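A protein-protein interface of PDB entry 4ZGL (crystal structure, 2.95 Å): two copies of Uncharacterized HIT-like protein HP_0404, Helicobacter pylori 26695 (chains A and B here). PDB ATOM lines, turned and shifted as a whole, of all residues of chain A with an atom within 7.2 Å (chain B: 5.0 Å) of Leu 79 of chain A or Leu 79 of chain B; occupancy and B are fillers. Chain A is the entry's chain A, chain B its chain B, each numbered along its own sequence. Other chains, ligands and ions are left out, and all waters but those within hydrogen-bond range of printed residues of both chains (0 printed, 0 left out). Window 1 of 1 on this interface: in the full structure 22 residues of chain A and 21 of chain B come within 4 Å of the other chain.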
ATOM      1  N   VAL A  39     -17.522  28.866  -5.266  1.00  0.00           N
ATOM      2  CA  VAL A  39     -18.804  29.503  -5.572  1.00  0.00           C
ATOM      3  C   VAL A  39     -19.442  29.980  -4.275  1.00  0.00           C
ATOM      4  O   VAL A  39     -19.672  29.179  -3.363  1.00  0.00           O
ATOM      5  CB  VAL A  39     -19.772  28.540  -6.280  1.00  0.00           C
ATOM      6  CG1 VAL A  39     -21.087  29.243  -6.595  1.00  0.00           C
ATOM      7  CG2 VAL A  39     -19.129  27.989  -7.542  1.00  0.00           C
ATOM      8  N   PHE A  48     -23.951  25.638   4.636  1.00  0.00           N
ATOM      9  CA  PHE A  48     -25.008  25.004   3.858  1.00  0.00           C
ATOM     10  C   PHE A  48     -26.317  24.913   4.633  1.00  0.00           C
ATOM     11  O   PHE A  48     -27.395  25.048   4.062  1.00  0.00           O
ATOM     12  CB  PHE A  48     -24.576  23.615   3.403  1.00  0.00           C
ATOM     13  CG  PHE A  48     -25.532  22.968   2.447  1.00  0.00           C
ATOM     14  CD1 PHE A  48     -25.599  23.381   1.121  1.00  0.00           C
ATOM     15  CD2 PHE A  48     -26.375  21.949   2.870  1.00  0.00           C
ATOM     16  CE1 PHE A  48     -26.488  22.787   0.234  1.00  0.00           C
ATOM     17  CE2 PHE A  48     -27.263  21.351   1.991  1.00  0.00           C
ATOM     18  CZ  PHE A  48     -27.318  21.770   0.671  1.00  0.00           C
ATOM     19  N   MET A  56     -30.635  27.565  -3.455  1.00  0.00           N
ATOM     20  CA  MET A  56     -29.741  26.484  -3.854  1.00  0.00           C
ATOM     21  C   MET A  56     -30.112  25.969  -5.244  1.00  0.00           C
ATOM     22  O   MET A  56     -29.261  25.442  -5.960  1.00  0.00           O
ATOM     23  CB  MET A  56     -29.799  25.360  -2.823  1.00  0.00           C
ATOM     24  CG  MET A  56     -28.801  24.239  -3.039  1.00  0.00           C
ATOM     25  SD  MET A  56     -27.061  24.732  -3.070  1.00  0.00           S
ATOM     26  CE  MET A  56     -26.246  23.237  -3.660  1.00  0.00           C
ATOM     27  N   THR A  60     -27.345  26.030  -8.090  1.00  0.00           N
ATOM     28  CA  THR A  60     -27.121  24.863  -8.937  1.00  0.00           C
ATOM     29  C   THR A  60     -27.030  25.290 -10.398  1.00  0.00           C
ATOM     30  O   THR A  60     -26.153  24.841 -11.141  1.00  0.00           O
ATOM     31  CB  THR A  60     -28.269  23.852  -8.780  1.00  0.00           C
ATOM     32  OG1 THR A  60     -28.345  23.438  -7.412  1.00  0.00           O
ATOM     33  CG2 THR A  60     -28.066  22.636  -9.674  1.00  0.00           C
ATOM     34  N   ILE A  63     -23.789  27.070 -10.761  1.00  0.00           N
ATOM     35  CA  ILE A  63     -22.675  26.116 -10.750  1.00  0.00           C
ATOM     36  C   ILE A  63     -22.446  25.508 -12.133  1.00  0.00           C
ATOM     37  O   ILE A  63     -21.301  25.360 -12.561  1.00  0.00           O
ATOM     38  CB  ILE A  63     -22.883  25.003  -9.696  1.00  0.00           C
ATOM     39  CG1 ILE A  63     -22.657  25.573  -8.294  1.00  0.00           C
ATOM     40  CG2 ILE A  63     -21.931  23.835  -9.932  1.00  0.00           C
ATOM     41  CD1 ILE A  63     -23.170  24.695  -7.174  1.00  0.00           C
ATOM     42  N   PHE A  64     -23.533  25.183 -12.829  1.00  0.00           N
ATOM     43  CA  PHE A  64     -23.441  24.688 -14.200  1.00  0.00           C
ATOM     44  C   PHE A  64     -22.774  25.716 -15.113  1.00  0.00           C
ATOM     45  O   PHE A  64     -22.019  25.357 -16.016  1.00  0.00           O
ATOM     46  CB  PHE A  64     -24.825  24.326 -14.759  1.00  0.00           C
ATOM     47  CG  PHE A  64     -25.521  23.204 -14.025  1.00  0.00           C
ATOM     48  CD1 PHE A  64     -24.813  22.121 -13.514  1.00  0.00           C
ATOM     49  CD2 PHE A  64     -26.902  23.218 -13.875  1.00  0.00           C
ATOM     50  CE1 PHE A  64     -25.469  21.095 -12.850  1.00  0.00           C
ATOM     51  CE2 PHE A  64     -27.562  22.193 -13.212  1.00  0.00           C
ATOM     52  CZ  PHE A  64     -26.844  21.131 -12.700  1.00  0.00           C
ATOM     53  N   VAL A  67     -18.708  25.717 -14.188  1.00  0.00           N
ATOM     54  CA  VAL A  67     -17.990  24.540 -14.702  1.00  0.00           C
ATOM     55  C   VAL A  67     -17.918  24.518 -16.222  1.00  0.00           C
ATOM     56  O   VAL A  67     -16.969  23.979 -16.797  1.00  0.00           O
ATOM     57  CB  VAL A  67     -18.588  23.197 -14.226  1.00  0.00           C
ATOM     58  CG1 VAL A  67     -18.392  23.032 -12.727  1.00  0.00           C
ATOM     59  CG2 VAL A  67     -20.056  23.058 -14.620  1.00  0.00           C
ATOM     60  N   TYR A  77     -15.536  16.875 -12.458  1.00  0.00           N
ATOM     61  CA  TYR A  77     -15.239  17.750 -11.328  1.00  0.00           C
ATOM     62  C   TYR A  77     -15.881  17.270 -10.033  1.00  0.00           C
ATOM     63  O   TYR A  77     -16.829  16.487 -10.048  1.00  0.00           O
ATOM     64  CB  TYR A  77     -15.698  19.174 -11.631  1.00  0.00           C
ATOM     65  CG  TYR A  77     -17.190  19.328 -11.792  1.00  0.00           C
ATOM     66  CD1 TYR A  77     -17.800  19.106 -13.020  1.00  0.00           C
ATOM     67  CD2 TYR A  77     -17.991  19.713 -10.716  1.00  0.00           C
ATOM     68  CE1 TYR A  77     -19.168  19.252 -13.174  1.00  0.00           C
ATOM     69  CE2 TYR A  77     -19.359  19.862 -10.859  1.00  0.00           C
ATOM     70  CZ  TYR A  77     -19.942  19.631 -12.090  1.00  0.00           C
ATOM     71  OH  TYR A  77     -21.298  19.778 -12.242  1.00  0.00           O
ATOM     72  N   LYS A  78     -15.344  17.750  -8.914  1.00  0.00           N
ATOM     73  CA  LYS A  78     -15.880  17.452  -7.590  1.00  0.00           C
ATOM     74  C   LYS A  78     -16.631  18.664  -7.071  1.00  0.00           C
ATOM     75  O   LYS A  78     -16.219  19.804  -7.300  1.00  0.00           O
ATOM     76  CB  LYS A  78     -14.752  17.109  -6.619  1.00  0.00           C
ATOM     77  CG  LYS A  78     -13.842  15.989  -7.088  1.00  0.00           C
ATOM     78  CD  LYS A  78     -12.807  15.631  -6.032  1.00  0.00           C
ATOM     79  CE  LYS A  78     -11.784  14.648  -6.581  1.00  0.00           C
ATOM     80  NZ  LYS A  78     -11.235  13.750  -5.529  1.00  0.00           N
ATOM     81  N   LEU A  79     -17.729  18.410  -6.369  1.00  0.00           N
ATOM     82  CA  LEU A  79     -18.480  19.461  -5.692  1.00  0.00           C
ATOM     83  C   LEU A  79     -18.426  19.189  -4.195  1.00  0.00           C
ATOM     84  O   LEU A  79     -18.790  18.106  -3.750  1.00  0.00           O
ATOM     85  CB  LEU A  79     -19.935  19.524  -6.201  1.00  0.00           C
ATOM     86  CG  LEU A  79     -20.414  20.821  -6.847  1.00  0.00           C
ATOM     87  CD1 LEU A  79     -21.932  20.833  -6.919  1.00  0.00           C
ATOM     88  CD2 LEU A  79     -19.912  22.078  -6.160  1.00  0.00           C
ATOM     89  N   LEU A  80     -17.948  20.166  -3.426  1.00  0.00           N
ATOM     90  CA  LEU A  80     -17.751  19.996  -1.988  1.00  0.00           C
ATOM     91  C   LEU A  80     -18.116  21.263  -1.229  1.00  0.00           C
ATOM     92  O   LEU A  80     -17.788  22.365  -1.657  1.00  0.00           O
ATOM     93  CB  LEU A  80     -16.293  19.640  -1.697  1.00  0.00           C
ATOM     94  CG  LEU A  80     -15.834  19.603  -0.234  1.00  0.00           C
ATOM     95  CD1 LEU A  80     -16.196  18.282   0.426  1.00  0.00           C
ATOM     96  CD2 LEU A  80     -14.334  19.843  -0.142  1.00  0.00           C
ATOM     97  N   THR A  81     -18.792  21.100  -0.095  1.00  0.00           N
ATOM     98  CA  THR A  81     -18.944  22.190   0.863  1.00  0.00           C
ATOM     99  C   THR A  81     -18.825  21.632   2.277  1.00  0.00           C
ATOM    100  O   THR A  81     -19.366  20.572   2.584  1.00  0.00           O
ATOM    101  CB  THR A  81     -20.264  22.965   0.663  1.00  0.00           C
ATOM    102  OG1 THR A  81     -20.301  24.087   1.550  1.00  0.00           O
ATOM    103  CG2 THR A  81     -21.479  22.080   0.904  1.00  0.00           C
ATOM    104  N   ASN A  82     -18.088  22.346   3.122  1.00  0.00           N
ATOM    105  CA  ASN A  82     -17.896  21.959   4.516  1.00  0.00           C
ATOM    106  C   ASN A  82     -18.836  22.745   5.414  1.00  0.00           C
ATOM    107  O   ASN A  82     -18.870  23.971   5.360  1.00  0.00           O
ATOM    108  CB  ASN A  82     -16.453  22.206   4.933  1.00  0.00           C
ATOM    109  CG  ASN A  82     -15.466  21.464   4.057  1.00  0.00           C
ATOM    110  OD1 ASN A  82     -14.675  22.071   3.336  1.00  0.00           O
ATOM    111  ND2 ASN A  82     -15.509  20.142   4.117  1.00  0.00           N
ATOM    112  N   VAL A  83     -19.603  22.029   6.225  1.00  0.00           N
ATOM    113  CA  VAL A  83     -20.572  22.647   7.107  1.00  0.00           C
ATOM    114  C   VAL A  83     -20.051  22.585   8.543  1.00  0.00           C
ATOM    115  O   VAL A  83     -20.101  21.543   9.194  1.00  0.00           O
ATOM    116  CB  VAL A  83     -21.939  21.956   6.990  1.00  0.00           C
ATOM    117  CG1 VAL A  83     -23.003  22.737   7.745  1.00  0.00           C
ATOM    118  CG2 VAL A  83     -22.331  21.821   5.528  1.00  0.00           C
ATOM    119  N   ALA A  87     -16.184  19.935  10.409  1.00  0.00           N
ATOM    120  CA  ALA A  87     -16.082  19.299   9.099  1.00  0.00           C
ATOM    121  C   ALA A  87     -15.025  19.975   8.226  1.00  0.00           C
ATOM    122  O   ALA A  87     -14.978  19.741   7.013  1.00  0.00           O
ATOM    123  CB  ALA A  87     -17.433  19.327   8.407  1.00  0.00           C
ATOM    124  N   PHE A  96     -18.920  26.597  -1.976  1.00  0.00           N
ATOM    125  CA  PHE A  96     -18.722  25.299  -2.589  1.00  0.00           C
ATOM    126  C   PHE A  96     -17.380  25.273  -3.300  1.00  0.00           C
ATOM    127  O   PHE A  96     -17.070  26.174  -4.080  1.00  0.00           O
ATOM    128  CB  PHE A  96     -19.835  25.001  -3.589  1.00  0.00           C
ATOM    129  CG  PHE A  96     -21.110  24.548  -2.953  1.00  0.00           C
ATOM    130  CD1 PHE A  96     -22.043  25.470  -2.507  1.00  0.00           C
ATOM    131  CD2 PHE A  96     -21.381  23.193  -2.801  1.00  0.00           C
ATOM    132  CE1 PHE A  96     -23.227  25.054  -1.916  1.00  0.00           C
ATOM    133  CE2 PHE A  96     -22.558  22.769  -2.215  1.00  0.00           C
ATOM    134  CZ  PHE A  96     -23.481  23.699  -1.771  1.00  0.00           C
ATOM    135  N   HIS A  97     -16.588  24.244  -3.019  1.00  0.00           N
ATOM    136  CA  HIS A  97     -15.355  24.000  -3.750  1.00  0.00           C
ATOM    137  C   HIS A  97     -15.700  23.276  -5.042  1.00  0.00           C
ATOM    138  O   HIS A  97     -16.485  22.325  -5.038  1.00  0.00           O
ATOM    139  CB  HIS A  97     -14.403  23.142  -2.925  1.00  0.00           C
ATOM    140  CG  HIS A  97     -13.971  23.780  -1.642  1.00  0.00           C
ATOM    141  ND1 HIS A  97     -12.721  24.330  -1.467  1.00  0.00           N
ATOM    142  CD2 HIS A  97     -14.620  23.949  -0.468  1.00  0.00           C
ATOM    143  CE1 HIS A  97     -12.614  24.809  -0.245  1.00  0.00           C
ATOM    144  NE2 HIS A  97     -13.754  24.594   0.383  1.00  0.00           N
ATOM    145  N   ILE A  98     -15.133  23.746  -6.148  1.00  0.00           N
ATOM    146  CA  ILE A  98     -15.195  23.023  -7.411  1.00  0.00           C
ATOM    147  C   ILE A  98     -13.777  22.621  -7.781  1.00  0.00           C
ATOM    148  O   ILE A  98     -12.962  23.467  -8.143  1.00  0.00           O
ATOM    149  CB  ILE A  98     -15.810  23.870  -8.532  1.00  0.00           C
ATOM    150  CG1 ILE A  98     -17.296  24.100  -8.247  1.00  0.00           C
ATOM    151  CG2 ILE A  98     -15.634  23.178  -9.883  1.00  0.00           C
ATOM    152  CD1 ILE A  98     -17.884  25.262  -9.013  1.00  0.00           C
ATOM    153  N   LEU A  99     -13.487  21.331  -7.657  1.00  0.00           N
ATOM    154  CA  LEU A  99     -12.178  20.788  -7.986  1.00  0.00           C
ATOM    155  C   LEU A  99     -12.285  19.950  -9.245  1.00  0.00           C
ATOM    156  O   LEU A  99     -13.355  19.443  -9.562  1.00  0.00           O
ATOM    157  CB  LEU A  99     -11.656  19.928  -6.834  1.00  0.00           C
ATOM    158  CG  LEU A  99     -11.587  20.608  -5.465  1.00  0.00           C
ATOM    159  CD1 LEU A  99     -11.266  19.600  -4.375  1.00  0.00           C
ATOM    160  CD2 LEU A  99     -10.555  21.724  -5.476  1.00  0.00           C
ATOM    161  N   PHE B  48     -24.379  15.114 -11.160  1.00  0.00           N
ATOM    162  CA  PHE B  48     -24.883  16.437 -10.806  1.00  0.00           C
ATOM    163  C   PHE B  48     -25.243  17.268 -12.035  1.00  0.00           C
ATOM    164  O   PHE B  48     -26.201  18.034 -12.014  1.00  0.00           O
ATOM    165  CB  PHE B  48     -23.865  17.186  -9.953  1.00  0.00           C
ATOM    166  CG  PHE B  48     -24.382  18.479  -9.392  1.00  0.00           C
ATOM    167  CD1 PHE B  48     -25.278  18.484  -8.330  1.00  0.00           C
ATOM    168  CD2 PHE B  48     -23.975  19.696  -9.927  1.00  0.00           C
ATOM    169  CE1 PHE B  48     -25.760  19.677  -7.812  1.00  0.00           C
ATOM    170  CE2 PHE B  48     -24.452  20.890  -9.412  1.00  0.00           C
ATOM    171  CZ  PHE B  48     -25.345  20.881  -8.355  1.00  0.00           C
ATOM    172  N   ILE B  63     -31.896  16.840   2.241  1.00  0.00           N
ATOM    173  CA  ILE B  63     -30.592  16.720   2.888  1.00  0.00           C
ATOM    174  C   ILE B  63     -30.641  17.235   4.323  1.00  0.00           C
ATOM    175  O   ILE B  63     -30.048  16.631   5.217  1.00  0.00           O
ATOM    176  CB  ILE B  63     -29.484  17.448   2.084  1.00  0.00           C
ATOM    177  CG1 ILE B  63     -29.144  16.641   0.828  1.00  0.00           C
ATOM    178  CG2 ILE B  63     -28.222  17.638   2.920  1.00  0.00           C
ATOM    179  CD1 ILE B  63     -28.347  17.401  -0.209  1.00  0.00           C
ATOM    180  N   TYR B  77     -20.759  18.445   9.226  1.00  0.00           N
ATOM    181  CA  TYR B  77     -20.715  17.424   8.188  1.00  0.00           C
ATOM    182  C   TYR B  77     -20.199  17.971   6.865  1.00  0.00           C
ATOM    183  O   TYR B  77     -20.212  19.181   6.629  1.00  0.00           O
ATOM    184  CB  TYR B  77     -22.104  16.823   7.982  1.00  0.00           C
ATOM    185  CG  TYR B  77     -23.142  17.794   7.455  1.00  0.00           C
ATOM    186  CD1 TYR B  77     -23.870  18.601   8.322  1.00  0.00           C
ATOM    187  CD2 TYR B  77     -23.411  17.888   6.089  1.00  0.00           C
ATOM    188  CE1 TYR B  77     -24.827  19.484   7.848  1.00  0.00           C
ATOM    189  CE2 TYR B  77     -24.366  18.771   5.606  1.00  0.00           C
ATOM    190  CZ  TYR B  77     -25.071  19.567   6.489  1.00  0.00           C
ATOM    191  OH  TYR B  77     -26.024  20.437   6.015  1.00  0.00           O
ATOM    192  N   LYS B  78     -19.750  17.060   6.006  1.00  0.00           N
ATOM    193  CA  LYS B  78     -19.283  17.400   4.667  1.00  0.00           C
ATOM    194  C   LYS B  78     -20.328  16.987   3.650  1.00  0.00           C
ATOM    195  O   LYS B  78     -20.986  15.961   3.808  1.00  0.00           O
ATOM    196  CB  LYS B  78     -17.977  16.677   4.357  1.00  0.00           C
ATOM    197  CG  LYS B  78     -16.875  16.906   5.377  1.00  0.00           C
ATOM    198  CD  LYS B  78     -15.573  16.244   4.952  1.00  0.00           C
ATOM    199  CE  LYS B  78     -14.533  16.322   6.062  1.00  0.00           C
ATOM    200  NZ  LYS B  78     -13.139  16.371   5.537  1.00  0.00           N
ATOM    201  N   LEU B  79     -20.485  17.802   2.613  1.00  0.00           N
ATOM    202  CA  LEU B  79     -21.361  17.477   1.495  1.00  0.00           C
ATOM    203  C   LEU B  79     -20.497  17.356   0.250  1.00  0.00           C
ATOM    204  O   LEU B  79     -19.765  18.284  -0.089  1.00  0.00           O
ATOM    205  CB  LEU B  79     -22.463  18.545   1.315  1.00  0.00           C
ATOM    206  CG  LEU B  79     -23.917  18.100   1.429  1.00  0.00           C
ATOM    207  CD1 LEU B  79     -24.835  19.166   0.844  1.00  0.00           C
ATOM    208  CD2 LEU B  79     -24.207  16.756   0.789  1.00  0.00           C
ATOM    209  N   LEU B  80     -20.578  16.212  -0.424  1.00  0.00           N
ATOM    210  CA  LEU B  80     -19.731  15.933  -1.580  1.00  0.00           C
ATOM    211  C   LEU B  80     -20.499  15.176  -2.651  1.00  0.00           C
ATOM    212  O   LEU B  80     -21.252  14.255  -2.346  1.00  0.00           O
ATOM    213  CB  LEU B  80     -18.516  15.107  -1.146  1.00  0.00           C
ATOM    214  CG  LEU B  80     -17.595  14.545  -2.237  1.00  0.00           C
ATOM    215  CD1 LEU B  80     -16.604  15.593  -2.714  1.00  0.00           C
ATOM    216  CD2 LEU B  80     -16.857  13.316  -1.723  1.00  0.00           C
ATOM    217  N   THR B  81     -20.289  15.551  -3.907  1.00  0.00           N
ATOM    218  CA  THR B  81     -20.718  14.723  -5.028  1.00  0.00           C
ATOM    219  C   THR B  81     -19.653  14.764  -6.120  1.00  0.00           C
ATOM    220  O   THR B  81     -19.096  15.820  -6.416  1.00  0.00           O
ATOM    221  CB  THR B  81     -22.103  15.138  -5.566  1.00  0.00           C
ATOM    222  OG1 THR B  81     -22.520  14.223  -6.583  1.00  0.00           O
ATOM    223  CG2 THR B  81     -22.084  16.552  -6.124  1.00  0.00           C
ATOM    224  N   PHE B  96     -24.984  12.176  -3.369  1.00  0.00           N
ATOM    225  CA  PHE B  96     -24.231  13.047  -2.485  1.00  0.00           C
ATOM    226  C   PHE B  96     -23.746  12.259  -1.282  1.00  0.00           C
ATOM    227  O   PHE B  96     -24.521  11.556  -0.639  1.00  0.00           O
ATOM    228  CB  PHE B  96     -25.097  14.209  -2.017  1.00  0.00           C
ATOM    229  CG  PHE B  96     -25.248  15.294  -3.033  1.00  0.00           C
ATOM    230  CD1 PHE B  96     -26.234  15.224  -4.004  1.00  0.00           C
ATOM    231  CD2 PHE B  96     -24.403  16.395  -3.019  1.00  0.00           C
ATOM    232  CE1 PHE B  96     -26.376  16.230  -4.944  1.00  0.00           C
ATOM    233  CE2 PHE B  96     -24.539  17.403  -3.956  1.00  0.00           C
ATOM    234  CZ  PHE B  96     -25.525  17.322  -4.919  1.00  0.00           C
ATOM    235  N   HIS B  97     -22.453  12.370  -0.993  1.00  0.00           N
ATOM    236  CA  HIS B  97     -21.883  11.811   0.224  1.00  0.00           C
ATOM    237  C   HIS B  97     -22.129  12.785   1.359  1.00  0.00           C
ATOM    238  O   HIS B  97     -21.924  13.991   1.205  1.00  0.00           O
ATOM    239  CB  HIS B  97     -20.382  11.591   0.068  1.00  0.00           C
ATOM    240  CG  HIS B  97     -20.023  10.616  -1.004  1.00  0.00           C
ATOM    241  ND1 HIS B  97     -19.610   9.332  -0.732  1.00  0.00           N
ATOM    242  CD2 HIS B  97     -20.013  10.736  -2.350  1.00  0.00           C
ATOM    243  CE1 HIS B  97     -19.359   8.701  -1.860  1.00  0.00           C
ATOM    244  NE2 HIS B  97     -19.597   9.533  -2.859  1.00  0.00           N
ATOM    245  N   ILE B  98     -22.597  12.264   2.488  1.00  0.00           N
ATOM    246  CA  ILE B  98     -22.675  13.040   3.717  1.00  0.00           C
ATOM    247  C   ILE B  98     -21.741  12.396   4.720  1.00  0.00           C
ATOM    248  O   ILE B  98     -22.018  11.311   5.226  1.00  0.00           O
ATOM    249  CB  ILE B  98     -24.102  13.094   4.280  1.00  0.00           C
ATOM    250  CG1 ILE B  98     -24.998  13.918   3.351  1.00  0.00           C
ATOM    251  CG2 ILE B  98     -24.106  13.697   5.682  1.00  0.00           C
ATOM    252  CD1 ILE B  98     -26.474  13.661   3.553  1.00  0.00           C
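Among the printed residues, pairs that only touch across the chains: Phe 48 of chain A with Ile 63 of chain B, Phe 48 of chain A with Tyr 77 of chain B, Phe 48 of chain A with Leu 79 of chain B, Thr 60 of chain A with Phe 48 of chain B, Ile 63 of chain A with Phe 48 of chain B, Phe 64 of chain A with Phe 48 of chain B, Tyr 77 of chain A with Phe 48 of chain B, Lys 78 of chain A with Thr 81 of chain B, Leu 79 of chain A with Phe 48 of chain B, Leu 79 of chain A with Leu 79 of chain B, Leu 79 of chain A with Leu 80 of chain B, Leu 80 of chain A with Leu 79 of chain B, Thr 81 of chain A with Lys 78 of chain B, Asn 82 of chain A with Lys 78 of chain B, Ala 87 of chain A with Tyr 77 of chain B and Ala 87 of chain A with Lys 78 of chain B.
Val 39 of chain A touches none of the printed residues of chain B. Of the printed residues of chain B, Thr 60 of chain A touches Phe 48. Of the printed residues of chain B, Lys 78 of chain A touches Thr 81 (3.8 Å). Of chain B, only Phe 48, Leu 79, Leu 80 and Thr 81 come within 4 Å of Leu 79 of chain A. Of chain A, only Phe 48 (3.5 Å), Leu 79 (3.8 Å), Leu 80 (3.3 Å) and Thr 81 (3.0 Å) come within 4 Å of Leu 79 of chain B. The nearest residue of chain A that does not touch Leu 79 of chain B is Asn 82 of chain A (5.2 Å).
The backbone NH (N) of Leu 79 of chain A is in hydrogen-bond range of the backbone carbonyl oxygen (O) of Thr 81 of chain B, 2.9 Å away. The backbone NH of Val 83 of chain A lies within hydrogen-bond range of the backbone carbonyl oxygen of Tyr 77 of chain B, at 2.9 Å. The backbone NH (N) of Thr 81 of chain A sits at hydrogen-bond distance from the backbone carbonyl oxygen (O) of Leu 79 of chain B.
Phe 48 of chain A touches Tyr 77 of chain B, and with the chains exchanged Tyr 77 of chain A touches Phe 48 of chain B. Phe 48 of chain A touches Leu 79 of chain B, and with the chains exchanged Leu 79 of chain A touches Phe 48 of chain B. Leu 79 of chain A touches Leu 80 of chain B, and with the chains exchanged Leu 80 of chain A touches Leu 79 of chain B. Leu 79 of chain A touches Thr 81 of chain B, and with the chains exchanged Thr 81 of chain A touches Leu 79 of chain B.
The backbone carbonyl oxygen of Ala 87 of chain A sits at hydrogen-bond distance from the side-chain amide nitrogen of Asn 82 of chain A (3.0 Å). The backbone carbonyl oxygen (O) of Met 56 of chain A is in hydrogen-bond range of the side-chain hydroxyl (OG1) of Thr 60 of chain A. O of Leu 80 of chain B is in hydrogen-bond range of N of His 97 of chain B (2.6 Å). The backbone NH (N) of His 97 of chain A is in hydrogen-bond range of the backbone carbonyl oxygen (O) of Leu 80 of chain A (2.6 Å). The backbone carbonyl oxygen of Leu 99 of chain A is in hydrogen-bond range of the backbone NH of Lys 78 of chain A (2.7 Å).
Hydrophobic or aromatic side chains of chain B that line the printed part of chain A: Phe 48, Ile 63, Tyr 77, Leu 79 and Leu 80. Printed residues of chain A that touch a printed residue of chain B: Phe 48, Thr 60, Ile 63, Phe 64, Tyr 77, Lys 78, Leu 79, Leu 80, Thr 81, Asn 82, Val 83 and Ala 87. Hydrophobic or aromatic side chains of chain A within 4 Å of the printed part of chain B: Phe 48, Ile 63, Phe 64, Tyr 77, Leu 79, Leu 80, Val 83 and Ala 87. Among the printed residues, 19 pairs touch across the chains.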
